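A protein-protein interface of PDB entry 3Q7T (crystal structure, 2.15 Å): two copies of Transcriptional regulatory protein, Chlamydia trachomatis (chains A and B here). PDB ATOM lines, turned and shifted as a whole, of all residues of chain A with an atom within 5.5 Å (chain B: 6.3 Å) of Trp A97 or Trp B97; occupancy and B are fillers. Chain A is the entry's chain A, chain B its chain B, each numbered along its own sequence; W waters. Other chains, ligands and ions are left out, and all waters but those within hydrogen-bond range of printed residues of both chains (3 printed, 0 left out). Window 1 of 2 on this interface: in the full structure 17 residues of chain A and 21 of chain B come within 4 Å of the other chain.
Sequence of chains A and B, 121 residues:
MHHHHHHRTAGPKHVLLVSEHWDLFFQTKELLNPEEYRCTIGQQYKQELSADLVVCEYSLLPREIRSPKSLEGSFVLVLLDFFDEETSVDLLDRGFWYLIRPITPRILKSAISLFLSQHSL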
ATOM      1  N   VAL A  76     -11.288  -3.843  25.581  1.00  0.00           N
ATOM      2  CA  VAL A  76     -11.550  -2.773  24.649  1.00  0.00           C
ATOM      3  C   VAL A  76     -10.699  -3.018  23.435  1.00  0.00           C
ATOM      4  O   VAL A  76      -9.528  -3.399  23.554  1.00  0.00           O
ATOM      5  CB  VAL A  76     -11.228  -1.408  25.269  1.00  0.00           C
ATOM      6  CG1 VAL A  76     -11.544  -0.272  24.294  1.00  0.00           C
ATOM      7  CG2 VAL A  76     -12.006  -1.228  26.561  1.00  0.00           C
ATOM      8  N   LEU A  77     -11.313  -2.864  22.265  1.00  0.00           N
ATOM      9  CA  LEU A  77     -10.581  -2.847  21.018  1.00  0.00           C
ATOM     10  C   LEU A  77     -10.687  -1.431  20.461  1.00  0.00           C
ATOM     11  O   LEU A  77     -11.786  -0.926  20.258  1.00  0.00           O
ATOM     12  CB  LEU A  77     -11.172  -3.846  20.037  1.00  0.00           C
ATOM     13  CG  LEU A  77     -10.595  -3.805  18.632  1.00  0.00           C
ATOM     14  CD1 LEU A  77      -9.117  -4.247  18.664  1.00  0.00           C
ATOM     15  CD2 LEU A  77     -11.422  -4.685  17.684  1.00  0.00           C
ATOM     16  N   VAL A  78      -9.547  -0.789  20.220  1.00  0.00           N
ATOM     17  CA  VAL A  78      -9.541   0.620  19.851  1.00  0.00           C
ATOM     18  C   VAL A  78      -9.342   0.792  18.355  1.00  0.00           C
ATOM     19  O   VAL A  78      -8.492   0.142  17.768  1.00  0.00           O
ATOM     20  CB  VAL A  78      -8.437   1.393  20.605  1.00  0.00           C
ATOM     21  CG1 VAL A  78      -8.497   2.879  20.277  1.00  0.00           C
ATOM     22  CG2 VAL A  78      -8.560   1.157  22.098  1.00  0.00           C
ATOM     23  N   LEU A  91      -1.535   2.551  24.308  1.00  0.00           N
ATOM     24  CA  LEU A  91      -2.715   1.687  24.264  1.00  0.00           C
ATOM     25  C   LEU A  91      -2.374   0.281  24.759  1.00  0.00           C
ATOM     26  O   LEU A  91      -3.081  -0.279  25.599  1.00  0.00           O
ATOM     27  CB  LEU A  91      -3.332   1.651  22.861  1.00  0.00           C
ATOM     28  CG  LEU A  91      -3.977   2.974  22.430  1.00  0.00           C
ATOM     29  CD1 LEU A  91      -4.443   2.930  20.983  1.00  0.00           C
ATOM     30  CD2 LEU A  91      -5.129   3.321  23.363  1.00  0.00           C
ATOM     31  N   LEU A  92      -1.276  -0.271  24.249  1.00  0.00           N
ATOM     32  CA  LEU A  92      -0.869  -1.643  24.560  1.00  0.00           C
ATOM     33  C   LEU A  92      -0.428  -1.830  26.011  1.00  0.00           C
ATOM     34  O   LEU A  92      -0.716  -2.863  26.623  1.00  0.00           O
ATOM     35  CB  LEU A  92       0.237  -2.104  23.612  1.00  0.00           C
ATOM     36  CG  LEU A  92      -0.034  -2.145  22.101  1.00  0.00           C
ATOM     37  CD1 LEU A  92       1.283  -2.362  21.361  1.00  0.00           C
ATOM     38  CD2 LEU A  92      -1.055  -3.232  21.711  1.00  0.00           C
ATOM     39  N   GLY A  95      -3.321  -2.098  28.029  1.00  0.00           N
ATOM     40  CA  GLY A  95      -3.938  -3.397  27.824  1.00  0.00           C
ATOM     41  C   GLY A  95      -5.008  -3.414  26.752  1.00  0.00           C
ATOM     42  O   GLY A  95      -5.888  -4.283  26.767  1.00  0.00           O
ATOM     43  N   PHE A  96      -4.935  -2.471  25.816  1.00  0.00           N
ATOM     44  CA  PHE A  96      -5.899  -2.431  24.715  1.00  0.00           C
ATOM     45  C   PHE A  96      -5.253  -2.831  23.391  1.00  0.00           C
ATOM     46  O   PHE A  96      -4.185  -2.323  23.049  1.00  0.00           O
ATOM     47  CB  PHE A  96      -6.503  -1.031  24.581  1.00  0.00           C
ATOM     48  CG  PHE A  96      -7.130  -0.510  25.850  1.00  0.00           C
ATOM     49  CD1 PHE A  96      -7.726  -1.375  26.758  1.00  0.00           C
ATOM     50  CD2 PHE A  96      -7.120   0.845  26.131  1.00  0.00           C
ATOM     51  CE1 PHE A  96      -8.310  -0.894  27.921  1.00  0.00           C
ATOM     52  CE2 PHE A  96      -7.694   1.338  27.295  1.00  0.00           C
ATOM     53  CZ  PHE A  96      -8.290   0.472  28.193  1.00  0.00           C
ATOM     54  N   TRP A  97      -5.895  -3.733  22.647  1.00  0.00           N
ATOM     55  CA  TRP A  97      -5.476  -4.007  21.273  1.00  0.00           C
ATOM     56  C   TRP A  97      -6.081  -2.949  20.392  1.00  0.00           C
ATOM     57  O   TRP A  97      -7.019  -2.262  20.792  1.00  0.00           O
ATOM     58  CB  TRP A  97      -5.909  -5.396  20.794  1.00  0.00           C
ATOM     59  CG  TRP A  97      -5.207  -5.861  19.514  1.00  0.00           C
ATOM     60  CD1 TRP A  97      -5.765  -6.023  18.264  1.00  0.00           C
ATOM     61  CD2 TRP A  97      -3.819  -6.220  19.378  1.00  0.00           C
ATOM     62  NE1 TRP A  97      -4.807  -6.471  17.371  1.00  0.00           N
ATOM     63  CE2 TRP A  97      -3.608  -6.593  18.028  1.00  0.00           C
ATOM     64  CE3 TRP A  97      -2.738  -6.267  20.269  1.00  0.00           C
ATOM     65  CZ2 TRP A  97      -2.362  -7.011  17.551  1.00  0.00           C
ATOM     66  CZ3 TRP A  97      -1.489  -6.679  19.789  1.00  0.00           C
ATOM     67  CH2 TRP A  97      -1.318  -7.049  18.441  1.00  0.00           C
ATOM     68  N   TYR A  98      -5.528  -2.774  19.202  1.00  0.00           N
ATOM     69  CA  TYR A  98      -6.042  -1.740  18.330  1.00  0.00           C
ATOM     70  C   TYR A  98      -6.053  -2.181  16.878  1.00  0.00           C
ATOM     71  O   TYR A  98      -5.327  -3.094  16.476  1.00  0.00           O
ATOM     72  CB  TYR A  98      -5.259  -0.431  18.505  1.00  0.00           C
ATOM     73  CG  TYR A  98      -3.791  -0.511  18.127  1.00  0.00           C
ATOM     74  CD1 TYR A  98      -3.385  -0.407  16.803  1.00  0.00           C
ATOM     75  CD2 TYR A  98      -2.817  -0.672  19.094  1.00  0.00           C
ATOM     76  CE1 TYR A  98      -2.030  -0.473  16.453  1.00  0.00           C
ATOM     77  CE2 TYR A  98      -1.472  -0.744  18.764  1.00  0.00           C
ATOM     78  CZ  TYR A  98      -1.081  -0.639  17.442  1.00  0.00           C
ATOM     79  OH  TYR A  98       0.259  -0.706  17.115  1.00  0.00           O
ATOM     80  N   LEU A  99      -6.896  -1.522  16.104  1.00  0.00           N
ATOM     81  CA  LEU A  99      -6.909  -1.688  14.664  1.00  0.00           C
ATOM     82  C   LEU A  99      -6.731  -0.322  14.056  1.00  0.00           C
ATOM     83  O   LEU A  99      -7.365   0.637  14.482  1.00  0.00           O
ATOM     84  CB  LEU A  99      -8.241  -2.271  14.182  1.00  0.00           C
ATOM     85  CG  LEU A  99      -8.616  -3.678  14.665  1.00  0.00           C
ATOM     86  CD1 LEU A  99     -10.010  -4.074  14.135  1.00  0.00           C
ATOM     87  CD2 LEU A  99      -7.554  -4.682  14.246  1.00  0.00           C
ATOM     88  N   ALA A 111     -12.241  -9.756  13.994  1.00  0.00           N
ATOM     89  CA  ALA A 111     -11.451  -9.355  15.162  1.00  0.00           C
ATOM     90  C   ALA A 111     -12.251  -9.515  16.456  1.00  0.00           C
ATOM     91  O   ALA A 111     -11.724  -9.938  17.473  1.00  0.00           O
ATOM     92  CB  ALA A 111     -10.966  -7.895  14.994  1.00  0.00           C
ATOM     93  N   ILE A 112     -13.526  -9.143  16.406  1.00  0.00           N
ATOM     94  CA  ILE A 112     -14.439  -9.355  17.511  1.00  0.00           C
ATOM     95  C   ILE A 112     -14.579 -10.856  17.830  1.00  0.00           C
ATOM     96  O   ILE A 112     -14.453 -11.241  18.976  1.00  0.00           O
ATOM     97  CB  ILE A 112     -15.819  -8.746  17.211  1.00  0.00           C
ATOM     98  CG1 ILE A 112     -15.722  -7.226  17.051  1.00  0.00           C
ATOM     99  CG2 ILE A 112     -16.834  -9.117  18.296  1.00  0.00           C
ATOM    100  CD1 ILE A 112     -16.986  -6.591  16.443  1.00  0.00           C
ATOM    101  N   LEU A 114     -12.499 -13.447  16.992  1.00  0.00           N
ATOM    102  CA  LEU A 114     -11.208 -13.890  17.513  1.00  0.00           C
ATOM    103  C   LEU A 114     -10.978 -13.453  18.955  1.00  0.00           C
ATOM    104  O   LEU A 114     -10.549 -14.236  19.799  1.00  0.00           O
ATOM    105  CB  LEU A 114     -10.068 -13.364  16.639  1.00  0.00           C
ATOM    106  CG  LEU A 114      -8.692 -13.938  16.963  1.00  0.00           C
ATOM    107  CD1 LEU A 114      -8.732 -15.475  17.036  1.00  0.00           C
ATOM    108  CD2 LEU A 114      -7.726 -13.474  15.917  1.00  0.00           C
ATOM    109  N   PHE A 115     -11.239 -12.189  19.242  1.00  0.00           N
ATOM    110  CA  PHE A 115     -10.963 -11.688  20.575  1.00  0.00           C
ATOM    111  C   PHE A 115     -11.828 -12.414  21.625  1.00  0.00           C
ATOM    112  O   PHE A 115     -11.342 -12.808  22.676  1.00  0.00           O
ATOM    113  CB  PHE A 115     -11.186 -10.184  20.651  1.00  0.00           C
ATOM    114  CG  PHE A 115     -10.824  -9.590  21.993  1.00  0.00           C
ATOM    115  CD1 PHE A 115      -9.567  -9.049  22.211  1.00  0.00           C
ATOM    116  CD2 PHE A 115     -11.735  -9.605  23.043  1.00  0.00           C
ATOM    117  CE1 PHE A 115      -9.223  -8.515  23.452  1.00  0.00           C
ATOM    118  CE2 PHE A 115     -11.400  -9.075  24.287  1.00  0.00           C
ATOM    119  CZ  PHE A 115     -10.139  -8.530  24.490  1.00  0.00           C
ATOM    120  N   GLN A 118     -10.928 -16.111  22.253  1.00  0.00           N
ATOM    121  CA  GLN A 118      -9.613 -16.310  22.886  1.00  0.00           C
ATOM    122  C   GLN A 118      -9.653 -16.180  24.417  1.00  0.00           C
ATOM    123  O   GLN A 118     -10.444 -15.411  24.966  1.00  0.00           O
ATOM    124  CB  GLN A 118      -8.552 -15.354  22.304  1.00  0.00           C
ATOM    125  CG  GLN A 118      -7.996 -15.768  20.934  1.00  0.00           C
ATOM    126  CD  GLN A 118      -6.765 -14.954  20.494  1.00  0.00           C
ATOM    127  OE1 GLN A 118      -6.544 -13.809  20.929  1.00  0.00           O
ATOM    128  NE2 GLN A 118      -5.954 -15.556  19.627  1.00  0.00           N
ATOM    129  N   PHE B  75      -0.606 -18.566  20.987  1.00  0.00           N
ATOM    130  CA  PHE B  75      -0.720 -17.220  20.402  1.00  0.00           C
ATOM    131  C   PHE B  75       0.206 -17.090  19.220  1.00  0.00           C
ATOM    132  O   PHE B  75       1.375 -17.507  19.285  1.00  0.00           O
ATOM    133  CB  PHE B  75      -0.361 -16.114  21.401  1.00  0.00           C
ATOM    134  CG  PHE B  75      -1.458 -15.766  22.360  1.00  0.00           C
ATOM    135  CD1 PHE B  75      -2.670 -15.274  21.899  1.00  0.00           C
ATOM    136  CD2 PHE B  75      -1.274 -15.915  23.727  1.00  0.00           C
ATOM    137  CE1 PHE B  75      -3.690 -14.952  22.786  1.00  0.00           C
ATOM    138  CE2 PHE B  75      -2.289 -15.593  24.621  1.00  0.00           C
ATOM    139  CZ  PHE B  75      -3.499 -15.111  24.150  1.00  0.00           C
ATOM    140  N   VAL B  76      -0.318 -16.491  18.153  1.00  0.00           N
ATOM    141  CA  VAL B  76       0.471 -16.137  16.988  1.00  0.00           C
ATOM    142  C   VAL B  76       0.182 -14.699  16.631  1.00  0.00           C
ATOM    143  O   VAL B  76      -0.968 -14.275  16.613  1.00  0.00           O
ATOM    144  CB  VAL B  76       0.161 -17.027  15.775  1.00  0.00           C
ATOM    145  CG1 VAL B  76       0.946 -16.544  14.550  1.00  0.00           C
ATOM    146  CG2 VAL B  76       0.520 -18.467  16.091  1.00  0.00           C
ATOM    147  N   LEU B  77       1.248 -13.943  16.400  1.00  0.00           N
ATOM    148  CA  LEU B  77       1.154 -12.569  15.955  1.00  0.00           C
ATOM    149  C   LEU B  77       1.882 -12.508  14.621  1.00  0.00           C
ATOM    150  O   LEU B  77       3.047 -12.873  14.531  1.00  0.00           O
ATOM    151  CB  LEU B  77       1.822 -11.649  16.983  1.00  0.00           C
ATOM    152  CG  LEU B  77       1.918 -10.157  16.677  1.00  0.00           C
ATOM    153  CD1 LEU B  77       0.525  -9.553  16.468  1.00  0.00           C
ATOM    154  CD2 LEU B  77       2.684  -9.443  17.807  1.00  0.00           C
ATOM    155  N   VAL B  78       1.191 -12.090  13.573  1.00  0.00           N
ATOM    156  CA  VAL B  78       1.807 -12.053  12.258  1.00  0.00           C
ATOM    157  C   VAL B  78       2.179 -10.617  11.877  1.00  0.00           C
ATOM    158  O   VAL B  78       1.399  -9.688  12.086  1.00  0.00           O
ATOM    159  CB  VAL B  78       0.859 -12.651  11.181  1.00  0.00           C
ATOM    160  CG1 VAL B  78       1.419 -12.439   9.809  1.00  0.00           C
ATOM    161  CG2 VAL B  78       0.627 -14.135  11.442  1.00  0.00           C
ATOM    162  N   LEU B  79       3.358 -10.442  11.291  1.00  0.00           N
ATOM    163  CA  LEU B  79       3.822  -9.103  10.949  1.00  0.00           C
ATOM    164  C   LEU B  79       3.712  -8.872   9.455  1.00  0.00           C
ATOM    165  O   LEU B  79       4.300  -9.593   8.657  1.00  0.00           O
ATOM    166  CB  LEU B  79       5.271  -8.882  11.414  1.00  0.00           C
ATOM    167  CG  LEU B  79       5.566  -9.133  12.894  1.00  0.00           C
ATOM    168  CD1 LEU B  79       7.007  -8.747  13.216  1.00  0.00           C
ATOM    169  CD2 LEU B  79       4.592  -8.397  13.820  1.00  0.00           C
ATOM    170  N   LEU B  91      -6.194 -13.912   7.979  1.00  0.00           N
ATOM    171  CA  LEU B  91      -5.377 -14.164   9.167  1.00  0.00           C
ATOM    172  C   LEU B  91      -6.233 -14.295  10.419  1.00  0.00           C
ATOM    173  O   LEU B  91      -6.035 -15.207  11.222  1.00  0.00           O
ATOM    174  CB  LEU B  91      -4.315 -13.064   9.359  1.00  0.00           C
ATOM    175  CG  LEU B  91      -3.190 -13.050   8.320  1.00  0.00           C
ATOM    176  CD1 LEU B  91      -2.348 -11.764   8.432  1.00  0.00           C
ATOM    177  CD2 LEU B  91      -2.317 -14.308   8.453  1.00  0.00           C
ATOM    178  N   LEU B  92      -7.177 -13.369  10.589  1.00  0.00           N
ATOM    179  CA  LEU B  92      -8.063 -13.360  11.747  1.00  0.00           C
ATOM    180  C   LEU B  92      -8.945 -14.622  11.844  1.00  0.00           C
ATOM    181  O   LEU B  92      -9.128 -15.171  12.931  1.00  0.00           O
ATOM    182  CB  LEU B  92      -8.939 -12.094  11.742  1.00  0.00           C
ATOM    183  CG  LEU B  92      -8.228 -10.746  11.892  1.00  0.00           C
ATOM    184  CD1 LEU B  92      -9.140  -9.574  11.489  1.00  0.00           C
ATOM    185  CD2 LEU B  92      -7.659 -10.569  13.313  1.00  0.00           C
ATOM    186  N   GLY B  95      -7.310 -17.541  13.170  1.00  0.00           N
ATOM    187  CA  GLY B  95      -6.954 -17.372  14.575  1.00  0.00           C
ATOM    188  C   GLY B  95      -5.684 -16.575  14.863  1.00  0.00           C
ATOM    189  O   GLY B  95      -5.154 -16.629  15.970  1.00  0.00           O
ATOM    190  N   PHE B  96      -5.195 -15.816  13.884  1.00  0.00           N
ATOM    191  CA  PHE B  96      -3.963 -15.046  14.082  1.00  0.00           C
ATOM    192  C   PHE B  96      -4.235 -13.557  14.196  1.00  0.00           C
ATOM    193  O   PHE B  96      -4.933 -12.992  13.362  1.00  0.00           O
ATOM    194  CB  PHE B  96      -3.001 -15.253  12.912  1.00  0.00           C
ATOM    195  CG  PHE B  96      -2.644 -16.687  12.660  1.00  0.00           C
ATOM    196  CD1 PHE B  96      -2.511 -17.580  13.708  1.00  0.00           C
ATOM    197  CD2 PHE B  96      -2.437 -17.141  11.370  1.00  0.00           C
ATOM    198  CE1 PHE B  96      -2.160 -18.910  13.468  1.00  0.00           C
ATOM    199  CE2 PHE B  96      -2.097 -18.458  11.128  1.00  0.00           C
ATOM    200  CZ  PHE B  96      -1.942 -19.337  12.169  1.00  0.00           C
ATOM    201  N   TRP B  97      -3.656 -12.909  15.203  1.00  0.00           N
ATOM    202  CA  TRP B  97      -3.635 -11.451  15.230  1.00  0.00           C
ATOM    203  C   TRP B  97      -2.522 -10.958  14.313  1.00  0.00           C
ATOM    204  O   TRP B  97      -1.613 -11.716  13.985  1.00  0.00           O
ATOM    205  CB  TRP B  97      -3.386 -10.942  16.640  1.00  0.00           C
ATOM    206  CG  TRP B  97      -4.550 -11.116  17.499  1.00  0.00           C
ATOM    207  CD1 TRP B  97      -4.683 -11.985  18.545  1.00  0.00           C
ATOM    208  CD2 TRP B  97      -5.798 -10.421  17.388  1.00  0.00           C
ATOM    209  NE1 TRP B  97      -5.941 -11.864  19.102  1.00  0.00           N
ATOM    210  CE2 TRP B  97      -6.643 -10.910  18.410  1.00  0.00           C
ATOM    211  CE3 TRP B  97      -6.287  -9.435  16.519  1.00  0.00           C
ATOM    212  CZ2 TRP B  97      -7.954 -10.444  18.587  1.00  0.00           C
ATOM    213  CZ3 TRP B  97      -7.582  -8.967  16.702  1.00  0.00           C
ATOM    214  CH2 TRP B  97      -8.401  -9.473  17.728  1.00  0.00           C
ATOM    215  N   TYR B  98      -2.579  -9.700  13.892  1.00  0.00           N
ATOM    216  CA  TYR B  98      -1.492  -9.179  13.088  1.00  0.00           C
ATOM    217  C   TYR B  98      -1.077  -7.779  13.492  1.00  0.00           C
ATOM    218  O   TYR B  98      -1.739  -7.109  14.293  1.00  0.00           O
ATOM    219  CB  TYR B  98      -1.828  -9.224  11.586  1.00  0.00           C
ATOM    220  CG  TYR B  98      -3.090  -8.474  11.224  1.00  0.00           C
ATOM    221  CD1 TYR B  98      -3.073  -7.097  11.063  1.00  0.00           C
ATOM    222  CD2 TYR B  98      -4.311  -9.146  11.057  1.00  0.00           C
ATOM    223  CE1 TYR B  98      -4.222  -6.394  10.739  1.00  0.00           C
ATOM    224  CE2 TYR B  98      -5.471  -8.450  10.736  1.00  0.00           C
ATOM    225  CZ  TYR B  98      -5.417  -7.069  10.576  1.00  0.00           C
ATOM    226  OH  TYR B  98      -6.548  -6.349  10.245  1.00  0.00           O
ATOM    227  N   LEU B  99       0.061  -7.365  12.948  1.00  0.00           N
ATOM    228  CA  LEU B  99       0.484  -5.979  13.013  1.00  0.00           C
ATOM    229  C   LEU B  99       0.995  -5.603  11.653  1.00  0.00           C
ATOM    230  O   LEU B  99       1.755  -6.348  11.031  1.00  0.00           O
ATOM    231  CB  LEU B  99       1.585  -5.774  14.049  1.00  0.00           C
ATOM    232  CG  LEU B  99       1.132  -5.677  15.501  1.00  0.00           C
ATOM    233  CD1 LEU B  99       2.356  -5.464  16.402  1.00  0.00           C
ATOM    234  CD2 LEU B  99       0.120  -4.550  15.677  1.00  0.00           C
ATOM    235  N   ALA B 111       3.266  -5.340  22.768  1.00  0.00           N
ATOM    236  CA  ALA B 111       2.393  -6.371  22.202  1.00  0.00           C
ATOM    237  C   ALA B 111       2.640  -7.737  22.817  1.00  0.00           C
ATOM    238  O   ALA B 111       1.703  -8.425  23.227  1.00  0.00           O
ATOM    239  CB  ALA B 111       2.548  -6.450  20.668  1.00  0.00           C
ATOM    240  N   LEU B 114       1.322  -7.661  26.262  1.00  0.00           N
ATOM    241  CA  LEU B 114      -0.136  -7.694  26.211  1.00  0.00           C
ATOM    242  C   LEU B 114      -0.649  -9.126  26.090  1.00  0.00           C
ATOM    243  O   LEU B 114      -1.488  -9.550  26.880  1.00  0.00           O
ATOM    244  CB  LEU B 114      -0.676  -6.845  25.060  1.00  0.00           C
ATOM    245  CG  LEU B 114      -2.208  -6.783  25.004  1.00  0.00           C
ATOM    246  CD1 LEU B 114      -2.756  -6.607  26.405  1.00  0.00           C
ATOM    247  CD2 LEU B 114      -2.677  -5.662  24.123  1.00  0.00           C
ATOM    248  N   PHE B 115      -0.129  -9.873  25.115  1.00  0.00           N
ATOM    249  CA  PHE B 115      -0.563 -11.250  24.883  1.00  0.00           C
ATOM    250  C   PHE B 115      -0.284 -12.173  26.055  1.00  0.00           C
ATOM    251  O   PHE B 115      -1.122 -13.003  26.409  1.00  0.00           O
ATOM    252  CB  PHE B 115       0.104 -11.830  23.639  1.00  0.00           C
ATOM    253  CG  PHE B 115      -0.501 -11.358  22.366  1.00  0.00           C
ATOM    254  CD1 PHE B 115      -1.745 -11.820  21.969  1.00  0.00           C
ATOM    255  CD2 PHE B 115       0.161 -10.441  21.570  1.00  0.00           C
ATOM    256  CE1 PHE B 115      -2.319 -11.373  20.797  1.00  0.00           C
ATOM    257  CE2 PHE B 115      -0.403  -9.994  20.406  1.00  0.00           C
ATOM    258  CZ  PHE B 115      -1.647 -10.451  20.012  1.00  0.00           C
HETATM  259  O   HOH W   1      -3.505 -15.205  18.121  1.00  0.00           O
HETATM  260  O   HOH W   2      -4.890  -7.210  14.071  1.00  0.00           O
HETATM  261  O   HOH W   3      -3.805  -4.447  14.518  1.00  0.00           O
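OE1 of Gln A118 is in hydrogen-bond range of NE1 of Trp B97 (2.7 Å).
N of Val A78 lies within hydrogen-bond range of O of Trp A97 (3.0 Å).
The backbone carbonyl oxygen (O) of Leu A91 lies within hydrogen-bond range of the backbone NH (N) of Phe A96.
O of Val B76 is in hydrogen-bond range of N of Trp B97, at 3.3 Å.
N of Val B78 is in hydrogen-bond range of O of Trp B97 (2.9 Å).
The backbone NH (N) of Leu B99 is in hydrogen-bond range of the backbone carbonyl oxygen (O) of Val B78.
N of Phe B96 is in hydrogen-bond range of O of Leu B91, 2.9 Å away.
Among the printed residues, merely in contact across the chains: Leu A92 with Ala B111 (3.8 Å), Leu A92 with Leu B114 (3.8 Å), Gly A95 with Leu B114 (3.7 Å), Phe A96 with Leu B114 (3.8 Å), Trp A97 with Leu B77 (3.7 Å), Trp A97 with Trp B97 (3.4 Å), Trp A97 with Tyr B98 (3.3 Å), Trp A97 with Leu B99 (3.97 Å), Trp A97 with Leu B114 (3.9 Å), Trp A97 with Phe B115 (3.5 Å), Ala A111 with Leu B92 (3.99 Å), Ala A111 with Trp B97 (3.4 Å), Leu A114 with Leu B92 (3.7 Å), Leu A114 with Gly B95 (3.6 Å), Leu A114 with Phe B96 (3.8 Å), Leu A114 with Trp B97 (3.7 Å), Phe A115 with Trp B97 (3.8 Å), Gln A118 with Phe B75 (3.6 Å) and Gln A118 with Gly B95 (3.9 Å).
Val A76 touches none of the printed residues of chain B.
Printed residues of chain B within 4 Å of Trp A97: Leu B77, Trp B97, Tyr B98, Leu B99, Leu B114 and Phe B115.
Printed residues of chain B within 4 Å of Leu A114: Leu B92, Gly B95, Phe B96 and Trp B97.
Val B76 touches none of the printed residues of chain A.
Printed residues of chain A within 4 Å of Gly B95: Leu A114 (3.6 Å) and Gln A118 (3.9 Å).
The nearest residue of chain B that does not touch Trp A97 is Ala B111 (4.1 Å).
The nearest printed residue of chain A that does not touch Leu B92 is Leu A99 (5.8 Å).
Of the 15 printed residues of chain A, 8 touch a printed residue of chain B.
Printed residues of chain A that touch a printed residue of chain B: Leu A92, Gly A95, Phe A96, Trp A97, Ala A111, Leu A114, Phe A115 and Gln A118.
Hydrophobic or aromatic side chains of chain A that line the printed part of chain B: Leu A92, Trp A97, Ala A111, Leu A114 and Phe A115.
Hydrophobic or aromatic side chains of chain B within 4 Å of the printed part of chain A: Phe B75, Leu B77, Leu B92, Trp B97, Leu B99, Leu B114 and Phe B115.
Among the printed residues, 20 pairs touch across the chains.
Among the printed residues, no Asp or Glu carboxylate lies within 4 Å of a Lys or Arg side-chain nitrogen of the other chain.
Leu A92 touches Leu B114, and with the chains exchanged Leu A114 touches Leu B92.
Gly A95 touches Leu B114, and with the chains exchanged Leu A114 touches Gly B95.
Trp B97 touches its own counterpart, Trp A97.
Trp A97 touches Leu B114, and with the chains exchanged Leu A114 touches Trp B97.
Positions printed for both chains: 76, 77, 78, 91, 92, 95, 96, 97, 98, 99, 111, 114 and 115.
Of the 20 pairs that touch across the chains among the printed residues, 13 have their exchanged pair printed and touching as well.
Water W3 lies within hydrogen-bond range of the backbone carbonyl oxygen (O) of Tyr A98 (2.8 Å) and the backbone carbonyl oxygen (O) of Tyr B98 (3.4 Å).
Water W1 lies within hydrogen-bond range of NE2 of Gln A118 (2.9 Å), O of Gly B95 (3.1 Å) and O of Val B76 (3.1 Å).
Water W2 bridges the backbone carbonyl oxygen (O) of Tyr B98 (3.2 Å) and the indole nitrogen (NE1) of Trp A97 (3.4 Å).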
